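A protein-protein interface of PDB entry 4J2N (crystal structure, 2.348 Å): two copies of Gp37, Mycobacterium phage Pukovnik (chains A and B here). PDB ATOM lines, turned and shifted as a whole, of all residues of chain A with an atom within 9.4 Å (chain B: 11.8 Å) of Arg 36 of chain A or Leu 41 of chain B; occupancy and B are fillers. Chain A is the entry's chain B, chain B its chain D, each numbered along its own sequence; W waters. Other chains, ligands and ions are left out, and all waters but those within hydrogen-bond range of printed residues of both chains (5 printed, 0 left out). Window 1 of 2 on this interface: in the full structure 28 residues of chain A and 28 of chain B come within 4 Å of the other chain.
Of the 16 printed residues of chain B, 9 touch a printed residue of chain A.
Hydrophobic or aromatic side chains of chain B that line the printed part of chain A: Leu 37, Leu 41, Ile 42 and Val 44.
Of the 16 printed residues of chain A, 11 touch a printed residue of chain B.
Water W4 lies within hydrogen-bond range of O of Leu 37 of chain B and N of Leu 41 of chain A.
Water W3 lies within hydrogen-bond range of the backbone carbonyl oxygen (O) of Leu 37 of chain A and the backbone NH (N) of Leu 41 of chain B.
Water W1 lies within hydrogen-bond range of the backbone NH of Ile 9 of chain A (2.7 Å) and the backbone carbonyl oxygen of Ile 42 of chain B (2.8 Å).
Water W2 bridges the backbone NH (N) of Ile 9 of chain B and the backbone carbonyl oxygen (O) of Ile 42 of chain A.
Water W5 bridges O of Arg 40 of chain A and NH1 of Arg 24 of chain B.
N of Val 35 of chain A is in hydrogen-bond range of O of Arg 43 of chain B, 2.8 Å away.
The backbone carbonyl oxygen (O) of Leu 41 of chain B sits at hydrogen-bond distance from the backbone NH (N) of Leu 37 of chain A.
The backbone carbonyl oxygen (O) of Leu 41 of chain A is in hydrogen-bond range of the backbone NH (N) of Leu 37 of chain B (3.0 Å).
The guanidinium group (NH2) of Arg 6 of chain A lies within salt-bridge range of the side-chain carboxylate (OE2) of Glu 45 of chain B (3.6 Å).
The backbone NH (N) of Val 44 of chain B is in hydrogen-bond range of the backbone carbonyl oxygen (O) of Ala 7 of chain A.
The side-chain carboxylate (OE1) of Glu 45 of chain B lies within salt-bridge range of the side-chain amino group (NZ) of Lys 33 of chain A (3.2 Å).
The guanidinium group (NH2) of Arg 36 of chain B is in hydrogen-bond range of the backbone carbonyl oxygen (O) of Gly 38 of chain B, 2.8 Å away.
The guanidinium group (NH2) of Arg 36 of chain A lies within hydrogen-bond range of the backbone carbonyl oxygen (O) of Gly 38 of chain A (3.0 Å).
Val 35 of chain A touches Leu 41 of chain B, and with the chains exchanged Leu 41 of chain A touches Val 35 of chain B.
Arg 36 of chain A touches Leu 41 of chain B, and with the chains exchanged Leu 41 of chain A touches Arg 36 of chain B.
Leu 37 of chain A touches Leu 41 of chain B, and with the chains exchanged Leu 41 of chain A touches Leu 37 of chain B.
Ile 42 of chain A touches Arg 24 of chain B, but with the chains exchanged Arg 24 of chain A does not touch Ile 42 of chain B (4.1 Å).
12 positions are printed for both chains.
Of the 21 pairs that touch across the chains among the printed residues, 8 have their exchanged pair printed and touching as well.
Arg 43 of chain B touches Arg 6 of chain A (CD to O, 3.5 Å).
Val 44 of chain B touches Arg 6 of chain A.
CA of Arg 43 of chain B touches O of Ala 7 of chain A (3.4 Å).
Ile 27 of chain A touches Val 44 of chain B.
Val 44 of chain B touches Lys 33 of chain A (CG1 to O, 3.5 Å).
O of Val 35 of chain A touches O of Leu 41 of chain B, at 3.9 Å.
CA of Ile 42 of chain B touches O of Val 35 of chain A, at 3.4 Å.
Val 35 of chain A touches Glu 45 of chain B (CG1 to OE2, 3.7 Å).
O of Leu 41 of chain A touches O of Val 35 of chain B (3.9 Å).
Val 35 of chain B touches Ile 42 of chain A.
Printed residues of chain B within 4 Å of Ile 27 of chain A: Val 44.
Ala 34 of chain A touches just one residue of chain B: Arg 43 (3.2 Å).
Arg 36 of chain A touches one residue of chain B.
Of chain B, only Leu 41 (3.0 Å) comes within 4 Å of Leu 37 of chain A.
No residue of chain B comes within 4 Å of Gly 38 of chain A.
No residue of chain B comes within 4 Å of Pro 39 of chain A.
No residue of chain B comes within 4 Å of Arg 40 of chain A.
Of the printed residues of chain A, Arg 24 of chain B touches Ile 42 (3.9 Å).
Gly 38 of chain B touches none of the printed residues of chain A.
Pro 39 of chain B touches none of the printed residues of chain A.
Of chain A, only Val 35 (3.9 Å), Arg 36 (3.3 Å) and Leu 37 (3.0 Å) come within 4 Å of Leu 41 of chain B.
Ile 42 of chain B touches one residue of chain A.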
ATOM      1  N   ARG A   6      -7.851 -33.925 -36.813  1.00  0.00           N
ATOM      2  CA  ARG A   6      -8.340 -33.213 -35.624  1.00  0.00           C
ATOM      3  C   ARG A   6      -7.206 -33.039 -34.597  1.00  0.00           C
ATOM      4  O   ARG A   6      -6.725 -34.008 -34.014  1.00  0.00           O
ATOM      5  CB  ARG A   6      -9.525 -33.964 -35.009  1.00  0.00           C
ATOM      6  CG  ARG A   6     -10.764 -34.048 -35.923  1.00  0.00           C
ATOM      7  CD  ARG A   6     -11.298 -32.664 -36.225  1.00  0.00           C
ATOM      8  NE  ARG A   6     -12.449 -32.674 -37.124  1.00  0.00           N
ATOM      9  CZ  ARG A   6     -12.379 -32.469 -38.438  1.00  0.00           C
ATOM     10  NH1 ARG A   6     -11.205 -32.240 -39.028  1.00  0.00           N
ATOM     11  NH2 ARG A   6     -13.486 -32.494 -39.168  1.00  0.00           N
ATOM     12  N   ALA A   7      -6.770 -31.802 -34.379  1.00  0.00           N
ATOM     13  CA  ALA A   7      -5.552 -31.566 -33.605  1.00  0.00           C
ATOM     14  C   ALA A   7      -5.814 -30.950 -32.225  1.00  0.00           C
ATOM     15  O   ALA A   7      -6.706 -30.114 -32.062  1.00  0.00           O
ATOM     16  CB  ALA A   7      -4.584 -30.686 -34.399  1.00  0.00           C
ATOM     17  N   SER A   8      -5.025 -31.354 -31.237  1.00  0.00           N
ATOM     18  CA  SER A   8      -5.159 -30.786 -29.905  1.00  0.00           C
ATOM     19  C   SER A   8      -4.901 -29.296 -29.985  1.00  0.00           C
ATOM     20  O   SER A   8      -4.257 -28.815 -30.917  1.00  0.00           O
ATOM     21  CB  SER A   8      -4.148 -31.413 -28.945  1.00  0.00           C
ATOM     22  OG  SER A   8      -2.862 -30.816 -29.088  1.00  0.00           O
ATOM     23  N   ILE A   9      -5.393 -28.567 -29.001  1.00  0.00           N
ATOM     24  CA  ILE A   9      -5.067 -27.160 -28.881  1.00  0.00           C
ATOM     25  C   ILE A   9      -3.551 -26.990 -28.811  1.00  0.00           C
ATOM     26  O   ILE A   9      -2.989 -26.087 -29.438  1.00  0.00           O
ATOM     27  CB  ILE A   9      -5.731 -26.546 -27.643  1.00  0.00           C
ATOM     28  CG1 ILE A   9      -7.249 -26.444 -27.869  1.00  0.00           C
ATOM     29  CG2 ILE A   9      -5.137 -25.181 -27.336  1.00  0.00           C
ATOM     30  CD1 ILE A   9      -8.054 -26.199 -26.608  1.00  0.00           C
ATOM     31  N   ARG A  24      -7.139 -20.630 -28.280  1.00  0.00           N
ATOM     32  CA  ARG A  24      -8.453 -20.584 -27.661  1.00  0.00           C
ATOM     33  C   ARG A  24      -9.180 -19.296 -28.047  1.00  0.00           C
ATOM     34  O   ARG A  24     -10.366 -19.332 -28.363  1.00  0.00           O
ATOM     35  CB  ARG A  24      -8.355 -20.779 -26.141  1.00  0.00           C
ATOM     36  CG  ARG A  24      -7.502 -22.001 -25.752  1.00  0.00           C
ATOM     37  CD  ARG A  24      -7.594 -22.365 -24.267  1.00  0.00           C
ATOM     38  NE  ARG A  24      -8.948 -22.782 -23.936  1.00  0.00           N
ATOM     39  CZ  ARG A  24      -9.305 -24.024 -23.619  1.00  0.00           C
ATOM     40  NH1 ARG A  24      -8.397 -24.996 -23.559  1.00  0.00           N
ATOM     41  NH2 ARG A  24     -10.581 -24.285 -23.348  1.00  0.00           N
ATOM     42  N   ILE A  27     -10.293 -19.737 -31.819  1.00  0.00           N
ATOM     43  CA  ILE A  27     -11.488 -20.562 -31.828  1.00  0.00           C
ATOM     44  C   ILE A  27     -12.715 -19.731 -31.434  1.00  0.00           C
ATOM     45  O   ILE A  27     -13.705 -19.665 -32.170  1.00  0.00           O
ATOM     46  CB  ILE A  27     -11.331 -21.735 -30.860  1.00  0.00           C
ATOM     47  CG1 ILE A  27     -10.221 -22.659 -31.353  1.00  0.00           C
ATOM     48  CG2 ILE A  27     -12.645 -22.504 -30.725  1.00  0.00           C
ATOM     49  CD1 ILE A  27      -9.974 -23.833 -30.436  1.00  0.00           C
ATOM     50  N   LYS A  33     -11.836 -23.459 -36.473  1.00  0.00           N
ATOM     51  CA  LYS A  33     -12.984 -24.302 -36.152  1.00  0.00           C
ATOM     52  C   LYS A  33     -12.506 -25.400 -35.225  1.00  0.00           C
ATOM     53  O   LYS A  33     -11.431 -25.970 -35.430  1.00  0.00           O
ATOM     54  CB  LYS A  33     -13.612 -24.923 -37.399  1.00  0.00           C
ATOM     55  CG  LYS A  33     -14.124 -23.929 -38.430  1.00  0.00           C
ATOM     56  CD  LYS A  33     -14.698 -24.652 -39.653  1.00  0.00           C
ATOM     57  CE  LYS A  33     -15.801 -25.638 -39.247  1.00  0.00           C
ATOM     58  NZ  LYS A  33     -16.225 -26.531 -40.377  1.00  0.00           N
ATOM     59  N   ALA A  34     -13.302 -25.683 -34.197  1.00  0.00           N
ATOM     60  CA  ALA A  34     -12.959 -26.706 -33.223  1.00  0.00           C
ATOM     61  C   ALA A  34     -14.199 -27.495 -32.848  1.00  0.00           C
ATOM     62  O   ALA A  34     -15.315 -27.040 -33.051  1.00  0.00           O
ATOM     63  CB  ALA A  34     -12.325 -26.083 -31.994  1.00  0.00           C
ATOM     64  N   VAL A  35     -13.989 -28.697 -32.332  1.00  0.00           N
ATOM     65  CA  VAL A  35     -15.085 -29.533 -31.891  1.00  0.00           C
ATOM     66  C   VAL A  35     -14.778 -30.073 -30.496  1.00  0.00           C
ATOM     67  O   VAL A  35     -13.634 -30.021 -30.040  1.00  0.00           O
ATOM     68  CB  VAL A  35     -15.253 -30.736 -32.808  1.00  0.00           C
ATOM     69  CG1 VAL A  35     -15.734 -30.303 -34.183  1.00  0.00           C
ATOM     70  CG2 VAL A  35     -13.947 -31.483 -32.885  1.00  0.00           C
ATOM     71  N   ARG A  36     -15.801 -30.591 -29.825  1.00  0.00           N
ATOM     72  CA  ARG A  36     -15.595 -31.374 -28.619  1.00  0.00           C
ATOM     73  C   ARG A  36     -16.015 -32.800 -28.905  1.00  0.00           C
ATOM     74  O   ARG A  36     -16.896 -33.037 -29.730  1.00  0.00           O
ATOM     75  CB  ARG A  36     -16.412 -30.814 -27.456  1.00  0.00           C
ATOM     76  CG  ARG A  36     -17.926 -30.815 -27.685  1.00  0.00           C
ATOM     77  CD  ARG A  36     -18.652 -30.173 -26.518  1.00  0.00           C
ATOM     78  NE  ARG A  36     -20.026 -29.828 -26.873  1.00  0.00           N
ATOM     79  CZ  ARG A  36     -21.040 -30.684 -26.830  1.00  0.00           C
ATOM     80  NH1 ARG A  36     -22.251 -30.279 -27.176  1.00  0.00           N
ATOM     81  NH2 ARG A  36     -20.840 -31.941 -26.448  1.00  0.00           N
ATOM     82  N   LEU A  37     -15.397 -33.752 -28.223  1.00  0.00           N
ATOM     83  CA  LEU A  37     -15.717 -35.149 -28.454  1.00  0.00           C
ATOM     84  C   LEU A  37     -16.634 -35.699 -27.362  1.00  0.00           C
ATOM     85  O   LEU A  37     -16.284 -35.703 -26.175  1.00  0.00           O
ATOM     86  CB  LEU A  37     -14.444 -35.991 -28.511  1.00  0.00           C
ATOM     87  CG  LEU A  37     -13.250 -35.481 -29.319  1.00  0.00           C
ATOM     88  CD1 LEU A  37     -12.206 -36.577 -29.421  1.00  0.00           C
ATOM     89  CD2 LEU A  37     -13.651 -34.999 -30.698  1.00  0.00           C
ATOM     90  N   GLY A  38     -17.802 -36.176 -27.771  1.00  0.00           N
ATOM     91  CA  GLY A  38     -18.715 -36.834 -26.852  1.00  0.00           C
ATOM     92  C   GLY A  38     -19.656 -35.866 -26.168  1.00  0.00           C
ATOM     93  O   GLY A  38     -19.495 -34.648 -26.271  1.00  0.00           O
ATOM     94  N   PRO A  39     -20.658 -36.409 -25.473  1.00  0.00           N
ATOM     95  CA  PRO A  39     -21.633 -35.598 -24.738  1.00  0.00           C
ATOM     96  C   PRO A  39     -21.001 -34.958 -23.503  1.00  0.00           C
ATOM     97  O   PRO A  39     -20.117 -35.567 -22.886  1.00  0.00           O
ATOM     98  CB  PRO A  39     -22.659 -36.633 -24.282  1.00  0.00           C
ATOM     99  CG  PRO A  39     -21.858 -37.894 -24.135  1.00  0.00           C
ATOM    100  CD  PRO A  39     -20.892 -37.852 -25.300  1.00  0.00           C
ATOM    101  N   ARG A  40     -21.448 -33.753 -23.154  1.00  0.00           N
ATOM    102  CA  ARG A  40     -21.093 -33.139 -21.874  1.00  0.00           C
ATOM    103  C   ARG A  40     -21.873 -33.793 -20.719  1.00  0.00           C
ATOM    104  O   ARG A  40     -22.939 -34.389 -20.917  1.00  0.00           O
ATOM    105  CB  ARG A  40     -21.358 -31.629 -21.919  1.00  0.00           C
ATOM    106  CG  ARG A  40     -20.570 -30.915 -23.006  1.00  0.00           C
ATOM    107  CD  ARG A  40     -21.149 -29.543 -23.309  1.00  0.00           C
ATOM    108  NE  ARG A  40     -22.453 -29.663 -23.932  1.00  0.00           N
ATOM    109  CZ  ARG A  40     -23.210 -28.637 -24.301  1.00  0.00           C
ATOM    110  NH1 ARG A  40     -22.792 -27.392 -24.100  1.00  0.00           N
ATOM    111  NH2 ARG A  40     -24.384 -28.866 -24.878  1.00  0.00           N
ATOM    112  N   LEU A  41     -21.333 -33.712 -19.515  1.00  0.00           N
ATOM    113  CA  LEU A  41     -22.090 -34.129 -18.344  1.00  0.00           C
ATOM    114  C   LEU A  41     -22.777 -32.872 -17.832  1.00  0.00           C
ATOM    115  O   LEU A  41     -22.151 -32.037 -17.193  1.00  0.00           O
ATOM    116  CB  LEU A  41     -21.172 -34.760 -17.294  1.00  0.00           C
ATOM    117  CG  LEU A  41     -21.767 -35.134 -15.916  1.00  0.00           C
ATOM    118  CD1 LEU A  41     -23.005 -35.963 -16.055  1.00  0.00           C
ATOM    119  CD2 LEU A  41     -20.765 -35.896 -15.079  1.00  0.00           C
ATOM    120  N   ILE A  42     -24.056 -32.718 -18.160  1.00  0.00           N
ATOM    121  CA  ILE A  42     -24.779 -31.476 -17.901  1.00  0.00           C
ATOM    122  C   ILE A  42     -25.556 -31.545 -16.592  1.00  0.00           C
ATOM    123  O   ILE A  42     -26.070 -32.602 -16.225  1.00  0.00           O
ATOM    124  CB  ILE A  42     -25.708 -31.145 -19.084  1.00  0.00           C
ATOM    125  CG1 ILE A  42     -24.889 -31.069 -20.377  1.00  0.00           C
ATOM    126  CG2 ILE A  42     -26.426 -29.837 -18.876  1.00  0.00           C
ATOM    127  CD1 ILE A  42     -25.690 -30.698 -21.577  1.00  0.00           C
ATOM    128  N   ILE B   9     -30.578 -33.331 -16.576  1.00  0.00           N
ATOM    129  CA  ILE B   9     -31.621 -32.859 -17.474  1.00  0.00           C
ATOM    130  C   ILE B   9     -32.881 -33.693 -17.249  1.00  0.00           C
ATOM    131  O   ILE B   9     -33.976 -33.151 -17.109  1.00  0.00           O
ATOM    132  CB  ILE B   9     -31.149 -32.887 -18.944  1.00  0.00           C
ATOM    133  CG1 ILE B   9     -30.031 -31.863 -19.121  1.00  0.00           C
ATOM    134  CG2 ILE B   9     -32.296 -32.594 -19.917  1.00  0.00           C
ATOM    135  CD1 ILE B   9     -29.992 -31.185 -20.465  1.00  0.00           C
ATOM    136  N   ARG B  24     -33.833 -28.796 -22.490  1.00  0.00           N
ATOM    137  CA  ARG B  24     -32.756 -28.332 -23.364  1.00  0.00           C
ATOM    138  C   ARG B  24     -33.049 -26.992 -24.058  1.00  0.00           C
ATOM    139  O   ARG B  24     -32.160 -26.137 -24.166  1.00  0.00           O
ATOM    140  CB  ARG B  24     -32.425 -29.403 -24.397  1.00  0.00           C
ATOM    141  CG  ARG B  24     -31.783 -30.625 -23.780  1.00  0.00           C
ATOM    142  CD  ARG B  24     -31.091 -31.469 -24.823  1.00  0.00           C
ATOM    143  NE  ARG B  24     -30.098 -32.355 -24.216  1.00  0.00           N
ATOM    144  CZ  ARG B  24     -28.773 -32.164 -24.254  1.00  0.00           C
ATOM    145  NH1 ARG B  24     -27.975 -33.052 -23.672  1.00  0.00           N
ATOM    146  NH2 ARG B  24     -28.233 -31.107 -24.877  1.00  0.00           N
ATOM    147  N   ILE B  27     -32.725 -24.146 -21.429  1.00  0.00           N
ATOM    148  CA  ILE B  27     -31.314 -23.831 -21.213  1.00  0.00           C
ATOM    149  C   ILE B  27     -30.747 -22.969 -22.352  1.00  0.00           C
ATOM    150  O   ILE B  27     -30.024 -22.003 -22.101  1.00  0.00           O
ATOM    151  CB  ILE B  27     -30.473 -25.099 -21.063  1.00  0.00           C
ATOM    152  CG1 ILE B  27     -30.930 -25.887 -19.831  1.00  0.00           C
ATOM    153  CG2 ILE B  27     -29.001 -24.729 -20.957  1.00  0.00           C
ATOM    154  CD1 ILE B  27     -30.409 -27.310 -19.779  1.00  0.00           C
ATOM    155  N   ALA B  28     -31.096 -23.316 -23.593  1.00  0.00           N
ATOM    156  CA  ALA B  28     -30.662 -22.567 -24.778  1.00  0.00           C
ATOM    157  C   ALA B  28     -31.252 -21.159 -24.802  1.00  0.00           C
ATOM    158  O   ALA B  28     -30.635 -20.226 -25.314  1.00  0.00           O
ATOM    159  CB  ALA B  28     -31.050 -23.313 -26.048  1.00  0.00           C
ATOM    160  N   ALA B  34     -27.498 -23.806 -16.600  1.00  0.00           N
ATOM    161  CA  ALA B  34     -26.874 -25.120 -16.539  1.00  0.00           C
ATOM    162  C   ALA B  34     -25.360 -25.015 -16.534  1.00  0.00           C
ATOM    163  O   ALA B  34     -24.794 -23.978 -16.887  1.00  0.00           O
ATOM    164  CB  ALA B  34     -27.353 -25.996 -17.697  1.00  0.00           C
ATOM    165  N   VAL B  35     -24.713 -26.098 -16.115  1.00  0.00           N
ATOM    166  CA  VAL B  35     -23.268 -26.193 -16.116  1.00  0.00           C
ATOM    167  C   VAL B  35     -22.857 -27.547 -16.681  1.00  0.00           C
ATOM    168  O   VAL B  35     -23.642 -28.499 -16.665  1.00  0.00           O
ATOM    169  CB  VAL B  35     -22.673 -26.032 -14.686  1.00  0.00           C
ATOM    170  CG1 VAL B  35     -22.909 -24.618 -14.148  1.00  0.00           C
ATOM    171  CG2 VAL B  35     -23.241 -27.087 -13.734  1.00  0.00           C
ATOM    172  N   ARG B  36     -21.634 -27.616 -17.203  1.00  0.00           N
ATOM    173  CA  ARG B  36     -21.017 -28.874 -17.584  1.00  0.00           C
ATOM    174  C   ARG B  36     -19.947 -29.187 -16.547  1.00  0.00           C
ATOM    175  O   ARG B  36     -19.333 -28.277 -16.000  1.00  0.00           O
ATOM    176  CB  ARG B  36     -20.390 -28.778 -18.986  1.00  0.00           C
ATOM    177  CG  ARG B  36     -19.814 -27.409 -19.350  1.00  0.00           C
ATOM    178  CD  ARG B  36     -18.960 -27.453 -20.625  1.00  0.00           C
ATOM    179  NE  ARG B  36     -17.624 -27.906 -20.287  1.00  0.00           N
ATOM    180  CZ  ARG B  36     -16.541 -27.139 -20.269  1.00  0.00           C
ATOM    181  NH1 ARG B  36     -16.595 -25.860 -20.619  1.00  0.00           N
ATOM    182  NH2 ARG B  36     -15.389 -27.672 -19.910  1.00  0.00           N
ATOM    183  N   LEU B  37     -19.716 -30.465 -16.280  1.00  0.00           N
ATOM    184  CA  LEU B  37     -18.699 -30.857 -15.313  1.00  0.00           C
ATOM    185  C   LEU B  37     -17.352 -31.274 -15.962  1.00  0.00           C
ATOM    186  O   LEU B  37     -17.305 -32.193 -16.779  1.00  0.00           O
ATOM    187  CB  LEU B  37     -19.226 -31.986 -14.423  1.00  0.00           C
ATOM    188  CG  LEU B  37     -20.618 -31.860 -13.781  1.00  0.00           C
ATOM    189  CD1 LEU B  37     -20.681 -32.691 -12.514  1.00  0.00           C
ATOM    190  CD2 LEU B  37     -20.978 -30.421 -13.484  1.00  0.00           C
ATOM    191  N   GLY B  38     -16.262 -30.606 -15.584  1.00  0.00           N
ATOM    192  CA  GLY B  38     -14.949 -30.966 -16.086  1.00  0.00           C
ATOM    193  C   GLY B  38     -14.642 -30.417 -17.477  1.00  0.00           C
ATOM    194  O   GLY B  38     -15.513 -29.863 -18.151  1.00  0.00           O
ATOM    195  N   PRO B  39     -13.385 -30.559 -17.912  1.00  0.00           N
ATOM    196  CA  PRO B  39     -12.956 -30.035 -19.210  1.00  0.00           C
ATOM    197  C   PRO B  39     -13.504 -30.843 -20.370  1.00  0.00           C
ATOM    198  O   PRO B  39     -13.696 -32.050 -20.242  1.00  0.00           O
ATOM    199  CB  PRO B  39     -11.422 -30.193 -19.165  1.00  0.00           C
ATOM    200  CG  PRO B  39     -11.193 -31.285 -18.171  1.00  0.00           C
ATOM    201  CD  PRO B  39     -12.259 -31.090 -17.127  1.00  0.00           C
ATOM    202  N   ARG B  40     -13.735 -30.174 -21.494  1.00  0.00           N
ATOM    203  CA  ARG B  40     -14.069 -30.841 -22.755  1.00  0.00           C
ATOM    204  C   ARG B  40     -12.810 -31.412 -23.388  1.00  0.00           C
ATOM    205  O   ARG B  40     -11.708 -30.885 -23.196  1.00  0.00           O
ATOM    206  CB  ARG B  40     -14.706 -29.851 -23.732  1.00  0.00           C
ATOM    207  CG  ARG B  40     -16.004 -29.239 -23.224  1.00  0.00           C
ATOM    208  CD  ARG B  40     -16.343 -27.977 -23.987  1.00  0.00           C
ATOM    209  NE  ARG B  40     -15.364 -26.930 -23.741  1.00  0.00           N
ATOM    210  CZ  ARG B  40     -15.463 -25.686 -24.196  1.00  0.00           C
ATOM    211  NH1 ARG B  40     -16.502 -25.332 -24.937  1.00  0.00           N
ATOM    212  NH2 ARG B  40     -14.513 -24.798 -23.914  1.00  0.00           N
ATOM    213  N   LEU B  41     -12.965 -32.496 -24.133  1.00  0.00           N
ATOM    214  CA  LEU B  41     -11.876 -32.974 -24.958  1.00  0.00           C
ATOM    215  C   LEU B  41     -11.975 -32.234 -26.288  1.00  0.00           C
ATOM    216  O   LEU B  41     -12.878 -32.492 -27.086  1.00  0.00           O
ATOM    217  CB  LEU B  41     -11.981 -34.479 -25.151  1.00  0.00           C
ATOM    218  CG  LEU B  41     -10.877 -35.091 -26.006  1.00  0.00           C
ATOM    219  CD1 LEU B  41      -9.526 -34.551 -25.571  1.00  0.00           C
ATOM    220  CD2 LEU B  41     -10.929 -36.610 -25.903  1.00  0.00           C
ATOM    221  N   ILE B  42     -11.075 -31.283 -26.505  1.00  0.00           N
ATOM    222  CA  ILE B  42     -11.171 -30.400 -27.661  1.00  0.00           C
ATOM    223  C   ILE B  42     -10.192 -30.743 -28.772  1.00  0.00           C
ATOM    224  O   ILE B  42      -9.043 -31.101 -28.512  1.00  0.00           O
ATOM    225  CB  ILE B  42     -10.947 -28.944 -27.254  1.00  0.00           C
ATOM    226  CG1 ILE B  42     -11.836 -28.600 -26.066  1.00  0.00           C
ATOM    227  CG2 ILE B  42     -11.216 -28.013 -28.419  1.00  0.00           C
ATOM    228  CD1 ILE B  42     -12.107 -27.139 -25.926  1.00  0.00           C
ATOM    229  N   ARG B  43     -10.667 -30.610 -30.009  1.00  0.00           N
ATOM    230  CA  ARG B  43      -9.879 -30.824 -31.219  1.00  0.00           C
ATOM    231  C   ARG B  43     -10.145 -29.689 -32.206  1.00  0.00           C
ATOM    232  O   ARG B  43     -11.292 -29.249 -32.385  1.00  0.00           O
ATOM    233  CB  ARG B  43     -10.227 -32.166 -31.875  1.00  0.00           C
ATOM    234  CG  ARG B  43      -9.757 -33.388 -31.098  1.00  0.00           C
ATOM    235  CD  ARG B  43      -8.248 -33.359 -30.964  1.00  0.00           C
ATOM    236  NE  ARG B  43      -7.720 -34.410 -30.098  1.00  0.00           N
ATOM    237  CZ  ARG B  43      -7.361 -34.227 -28.827  1.00  0.00           C
ATOM    238  NH1 ARG B  43      -7.502 -33.039 -28.261  1.00  0.00           N
ATOM    239  NH2 ARG B  43      -6.859 -35.231 -28.122  1.00  0.00           N
ATOM    240  N   VAL B  44      -9.076 -29.221 -32.838  1.00  0.00           N
ATOM    241  CA  VAL B  44      -9.158 -28.175 -33.841  1.00  0.00           C
ATOM    242  C   VAL B  44      -9.159 -28.857 -35.204  1.00  0.00           C
ATOM    243  O   VAL B  44      -8.455 -29.856 -35.405  1.00  0.00           O
ATOM    244  CB  VAL B  44      -7.943 -27.219 -33.730  1.00  0.00           C
ATOM    245  CG1 VAL B  44      -8.020 -26.102 -34.760  1.00  0.00           C
ATOM    246  CG2 VAL B  44      -7.847 -26.654 -32.309  1.00  0.00           C
ATOM    247  N   GLU B  45      -9.953 -28.338 -36.130  1.00  0.00           N
ATOM    248  CA  GLU B  45     -10.032 -28.934 -37.464  1.00  0.00           C
ATOM    249  C   GLU B  45      -8.834 -28.509 -38.287  1.00  0.00           C
ATOM    250  O   GLU B  45      -8.632 -27.325 -38.538  1.00  0.00           O
ATOM    251  CB  GLU B  45     -11.348 -28.564 -38.154  1.00  0.00           C
ATOM    252  CG  GLU B  45     -12.573 -29.095 -37.409  1.00  0.00           C
ATOM    253  CD  GLU B  45     -13.870 -28.983 -38.198  1.00  0.00           C
ATOM    254  OE1 GLU B  45     -13.844 -28.403 -39.312  1.00  0.00           O
ATOM    255  OE2 GLU B  45     -14.915 -29.479 -37.701  1.00  0.00           O
HETATM  256  O   HOH W   1      -7.094 -29.663 -27.190  1.00  0.00           O
HETATM  257  O   HOH W   2     -28.073 -34.265 -17.760  1.00  0.00           O
HETATM  258  O   HOH W   3     -15.439 -33.713 -24.583  1.00  0.00           O
HETATM  259  O   HOH W   4     -18.561 -32.626 -19.066  1.00  0.00           O
HETATM  260  O   HOH W   5     -25.317 -34.703 -22.599  1.00  0.00           O
